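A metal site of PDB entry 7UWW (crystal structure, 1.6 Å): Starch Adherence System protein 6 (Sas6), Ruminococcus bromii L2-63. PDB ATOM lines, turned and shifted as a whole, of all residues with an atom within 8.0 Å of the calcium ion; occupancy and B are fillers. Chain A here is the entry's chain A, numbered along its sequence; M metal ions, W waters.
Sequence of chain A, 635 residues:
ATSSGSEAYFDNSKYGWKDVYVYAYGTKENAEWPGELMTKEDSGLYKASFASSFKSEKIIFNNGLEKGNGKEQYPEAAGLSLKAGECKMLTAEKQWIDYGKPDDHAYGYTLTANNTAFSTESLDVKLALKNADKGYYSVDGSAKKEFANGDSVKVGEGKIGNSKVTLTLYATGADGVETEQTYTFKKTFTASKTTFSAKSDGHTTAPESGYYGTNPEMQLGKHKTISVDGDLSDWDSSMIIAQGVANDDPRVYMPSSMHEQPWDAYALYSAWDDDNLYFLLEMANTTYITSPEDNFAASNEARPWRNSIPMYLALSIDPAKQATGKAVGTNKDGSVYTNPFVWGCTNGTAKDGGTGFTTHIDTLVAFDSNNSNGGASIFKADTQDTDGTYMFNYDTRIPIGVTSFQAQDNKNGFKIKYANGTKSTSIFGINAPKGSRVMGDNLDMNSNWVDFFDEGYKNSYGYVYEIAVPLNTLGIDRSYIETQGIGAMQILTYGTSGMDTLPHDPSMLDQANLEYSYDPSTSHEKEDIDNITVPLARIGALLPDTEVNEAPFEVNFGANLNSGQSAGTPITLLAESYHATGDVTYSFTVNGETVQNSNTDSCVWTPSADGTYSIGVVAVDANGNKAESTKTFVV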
ATOM      1  N   THR A 225      -1.257   2.434 -13.288  1.00  0.00           N
ATOM      2  CA  THR A 225      -1.157   3.857 -13.529  1.00  0.00           C
ATOM      3  C   THR A 225      -2.509   4.401 -14.001  1.00  0.00           C
ATOM      4  O   THR A 225      -3.086   3.911 -14.968  1.00  0.00           O
ATOM      5  CB  THR A 225      -0.036   4.138 -14.541  1.00  0.00           C
ATOM      6  OG1 THR A 225       1.258   3.844 -13.983  1.00  0.00           O
ATOM      7  CG2 THR A 225      -0.062   5.584 -14.908  1.00  0.00           C
ATOM      8  N   ILE A 226      -2.997   5.429 -13.322  1.00  0.00           N
ATOM      9  CA  ILE A 226      -4.307   6.041 -13.599  1.00  0.00           C
ATOM     10  C   ILE A 226      -4.065   7.337 -14.350  1.00  0.00           C
ATOM     11  O   ILE A 226      -3.093   8.039 -14.047  1.00  0.00           O
ATOM     12  CB  ILE A 226      -5.059   6.272 -12.271  1.00  0.00           C
ATOM     13  CG1 ILE A 226      -5.458   4.931 -11.631  1.00  0.00           C
ATOM     14  CG2 ILE A 226      -6.231   7.207 -12.453  1.00  0.00           C
ATOM     15  CD1 ILE A 226      -6.440   4.083 -12.442  1.00  0.00           C
ATOM     16  N   SER A 227      -4.950   7.679 -15.297  1.00  0.00           N
ATOM     17  CA  SER A 227      -4.923   8.983 -15.950  1.00  0.00           C
ATOM     18  C   SER A 227      -5.976   9.854 -15.283  1.00  0.00           C
ATOM     19  O   SER A 227      -7.181   9.565 -15.368  1.00  0.00           O
ATOM     20  CB  SER A 227      -5.185   8.874 -17.445  1.00  0.00           C
ATOM     21  OG  SER A 227      -5.142  10.156 -18.030  1.00  0.00           O
ATOM     22  N   VAL A 228      -5.530  10.894 -14.585  1.00  0.00           N
ATOM     23  CA  VAL A 228      -6.420  11.797 -13.855  1.00  0.00           C
ATOM     24  C   VAL A 228      -7.015  12.761 -14.874  1.00  0.00           C
ATOM     25  O   VAL A 228      -6.375  13.727 -15.260  1.00  0.00           O
ATOM     26  CB  VAL A 228      -5.690  12.545 -12.737  1.00  0.00           C
ATOM     27  CG1 VAL A 228      -6.542  13.498 -12.047  1.00  0.00           C
ATOM     28  CG2 VAL A 228      -5.182  11.497 -11.710  1.00  0.00           C
ATOM     29  N   ASP A 229      -8.216  12.499 -15.311  1.00  0.00           N
ATOM     30  CA  ASP A 229      -8.791  13.199 -16.456  1.00  0.00           C
ATOM     31  C   ASP A 229     -10.318  13.211 -16.444  1.00  0.00           C
ATOM     32  O   ASP A 229     -10.904  13.762 -17.369  1.00  0.00           O
ATOM     33  CB  ASP A 229      -8.290  12.536 -17.760  1.00  0.00           C
ATOM     34  CG  ASP A 229      -8.647  11.058 -17.851  1.00  0.00           C
ATOM     35  OD1 ASP A 229      -9.431  10.567 -17.003  1.00  0.00           O
ATOM     36  OD2 ASP A 229      -8.131  10.362 -18.765  1.00  0.00           O
ATOM     37  N   GLY A 230     -10.982  12.683 -15.414  1.00  0.00           N
ATOM     38  CA  GLY A 230     -12.426  12.637 -15.352  1.00  0.00           C
ATOM     39  C   GLY A 230     -13.045  11.524 -16.170  1.00  0.00           C
ATOM     40  O   GLY A 230     -14.251  11.291 -16.058  1.00  0.00           O
ATOM     41  N   ASP A 231     -12.269  10.827 -16.963  1.00  0.00           N
ATOM     42  CA  ASP A 231     -12.723   9.639 -17.668  1.00  0.00           C
ATOM     43  C   ASP A 231     -12.505   8.410 -16.779  1.00  0.00           C
ATOM     44  O   ASP A 231     -11.479   8.291 -16.125  1.00  0.00           O
ATOM     45  CB  ASP A 231     -11.945   9.478 -18.968  1.00  0.00           C
ATOM     46  CG  ASP A 231     -12.118   8.127 -19.556  1.00  0.00           C
ATOM     47  OD1 ASP A 231     -11.325   7.206 -19.240  1.00  0.00           O
ATOM     48  OD2 ASP A 231     -13.071   7.988 -20.372  1.00  0.00           O
ATOM     49  N   LEU A 232     -13.445   7.469 -16.822  1.00  0.00           N
ATOM     50  CA  LEU A 232     -13.488   6.394 -15.826  1.00  0.00           C
ATOM     51  C   LEU A 232     -13.064   5.037 -16.374  1.00  0.00           C
ATOM     52  O   LEU A 232     -13.182   4.030 -15.643  1.00  0.00           O
ATOM     53  CB  LEU A 232     -14.896   6.310 -15.250  1.00  0.00           C
ATOM     54  CG  LEU A 232     -15.465   7.612 -14.662  1.00  0.00           C
ATOM     55  CD1 LEU A 232     -16.919   7.496 -14.169  1.00  0.00           C
ATOM     56  CD2 LEU A 232     -14.555   8.098 -13.584  1.00  0.00           C
ATOM     57  N   SER A 233     -12.560   4.989 -17.611  1.00  0.00           N
ATOM     58  CA  SER A 233     -12.250   3.712 -18.257  1.00  0.00           C
ATOM     59  C   SER A 233     -11.056   3.015 -17.620  1.00  0.00           C
ATOM     60  O   SER A 233     -10.872   1.814 -17.845  1.00  0.00           O
ATOM     61  CB  SER A 233     -11.990   3.916 -19.755  1.00  0.00           C
ATOM     62  OG  SER A 233     -10.897   4.784 -19.995  1.00  0.00           O
ATOM     63  N   ASP A 234     -10.231   3.757 -16.868  1.00  0.00           N
ATOM     64  CA  ASP A 234      -9.065   3.198 -16.199  1.00  0.00           C
ATOM     65  C   ASP A 234      -9.357   2.610 -14.821  1.00  0.00           C
ATOM     66  O   ASP A 234      -8.446   2.097 -14.176  1.00  0.00           O
ATOM     67  CB  ASP A 234      -7.942   4.262 -16.088  1.00  0.00           C
ATOM     68  CG  ASP A 234      -8.432   5.659 -15.723  1.00  0.00           C
ATOM     69  OD1 ASP A 234      -9.646   5.932 -15.640  1.00  0.00           O
ATOM     70  OD2 ASP A 234      -7.552   6.548 -15.543  1.00  0.00           O
ATOM     71  N   TRP A 235     -10.598   2.638 -14.364  1.00  0.00           N
ATOM     72  CA  TRP A 235     -11.023   2.063 -13.076  1.00  0.00           C
ATOM     73  C   TRP A 235     -11.982   0.904 -13.324  1.00  0.00           C
ATOM     74  O   TRP A 235     -12.646   0.818 -14.354  1.00  0.00           O
ATOM     75  CB  TRP A 235     -11.703   3.127 -12.219  1.00  0.00           C
ATOM     76  CG  TRP A 235     -10.824   4.255 -11.823  1.00  0.00           C
ATOM     77  CD1 TRP A 235     -10.666   5.440 -12.458  1.00  0.00           C
ATOM     78  CD2 TRP A 235      -9.962   4.288 -10.670  1.00  0.00           C
ATOM     79  NE1 TRP A 235      -9.735   6.210 -11.793  1.00  0.00           N
ATOM     80  CE2 TRP A 235      -9.313   5.524 -10.676  1.00  0.00           C
ATOM     81  CE3 TRP A 235      -9.701   3.400  -9.629  1.00  0.00           C
ATOM     82  CZ2 TRP A 235      -8.418   5.904  -9.666  1.00  0.00           C
ATOM     83  CZ3 TRP A 235      -8.769   3.760  -8.649  1.00  0.00           C
ATOM     84  CH2 TRP A 235      -8.152   5.001  -8.674  1.00  0.00           C
ATOM     85  N   LEU A 280     -10.370   7.307  -6.957  1.00  0.00           N
ATOM     86  CA  LEU A 280     -11.626   7.696  -7.579  1.00  0.00           C
ATOM     87  C   LEU A 280     -12.681   7.755  -6.490  1.00  0.00           C
ATOM     88  O   LEU A 280     -12.846   6.781  -5.753  1.00  0.00           O
ATOM     89  CB  LEU A 280     -12.039   6.742  -8.685  1.00  0.00           C
ATOM     90  CG  LEU A 280     -13.457   6.918  -9.225  1.00  0.00           C
ATOM     91  CD1 LEU A 280     -13.541   8.249  -9.894  1.00  0.00           C
ATOM     92  CD2 LEU A 280     -13.828   5.791 -10.137  1.00  0.00           C
ATOM     93  N   LYS A 417      -9.297  16.101 -10.835  1.00  0.00           N
ATOM     94  CA  LYS A 417     -10.281  16.353 -11.898  1.00  0.00           C
ATOM     95  C   LYS A 417     -11.653  15.938 -11.356  1.00  0.00           C
ATOM     96  O   LYS A 417     -11.785  14.894 -10.689  1.00  0.00           O
ATOM     97  CB  LYS A 417      -9.935  15.603 -13.176  1.00  0.00           C
ATOM     98  CG  LYS A 417      -8.567  15.910 -13.741  1.00  0.00           C
ATOM     99  CD  LYS A 417      -8.589  17.231 -14.522  1.00  0.00           C
ATOM    100  CE  LYS A 417      -7.187  17.803 -14.761  1.00  0.00           C
ATOM    101  NZ  LYS A 417      -7.259  19.257 -15.164  1.00  0.00           N
ATOM    102  N   GLU A 466     -11.338  12.312  -9.582  1.00  0.00           N
ATOM    103  CA  GLU A 466     -10.132  11.514  -9.752  1.00  0.00           C
ATOM    104  C   GLU A 466      -8.983  12.330  -9.181  1.00  0.00           C
ATOM    105  O   GLU A 466      -8.852  13.513  -9.477  1.00  0.00           O
ATOM    106  CB  GLU A 466      -9.823  11.229 -11.231  1.00  0.00           C
ATOM    107  CG  GLU A 466     -10.452  10.048 -11.783  1.00  0.00           C
ATOM    108  CD  GLU A 466      -9.873   9.652 -13.133  1.00  0.00           C
ATOM    109  OE1 GLU A 466      -9.375   8.500 -13.296  1.00  0.00           O
ATOM    110  OE2 GLU A 466      -9.916  10.521 -14.029  1.00  0.00           O
HETATM  111 CA    CA M   1      -9.200   8.437 -15.663  1.00  0.00          CA
HETATM  112  O   HOH W   1      -8.922   7.781 -18.098  1.00  0.00           O
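The side-chain carboxylate of Asp 231 sits at hydrogen-bond distance from the side-chain hydroxyl of Ser 233, at 2.6 Å.
The side-chain carboxylate (OE1) of Glu 466 sits close to the indole nitrogen (NE1) of Trp 235.
OE2 of Glu 466 lies close to N of Gly 230 (2.8 Å).
The backbone NH (N) of Glu 466 is in hydrogen-bond range of the backbone carbonyl oxygen (O) of Lys 417 (2.8 Å).
The calcium ion is bound by the backbone carbonyl oxygen (O) of Asp 231, the backbone carbonyl oxygen (O) of Ser 227, the side-chain carboxylate (OE1) of Glu 466, the side-chain carboxylate (OD2) of Asp 234, the side-chain carboxylate (OD1) of Asp 229, water W1, the side-chain carboxylate (OD1) of Asp 234 and the side-chain carboxylate (OE2) of Glu 466.
Water W1 bridges OD1 of Asp 231 (2.7 Å) and OD2 of Asp 229 (2.8 Å).
Five residues have an atom within 4 Å of the calcium ion: Ser 227, Asp 229, Asp 231, Asp 234 and Glu 466.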
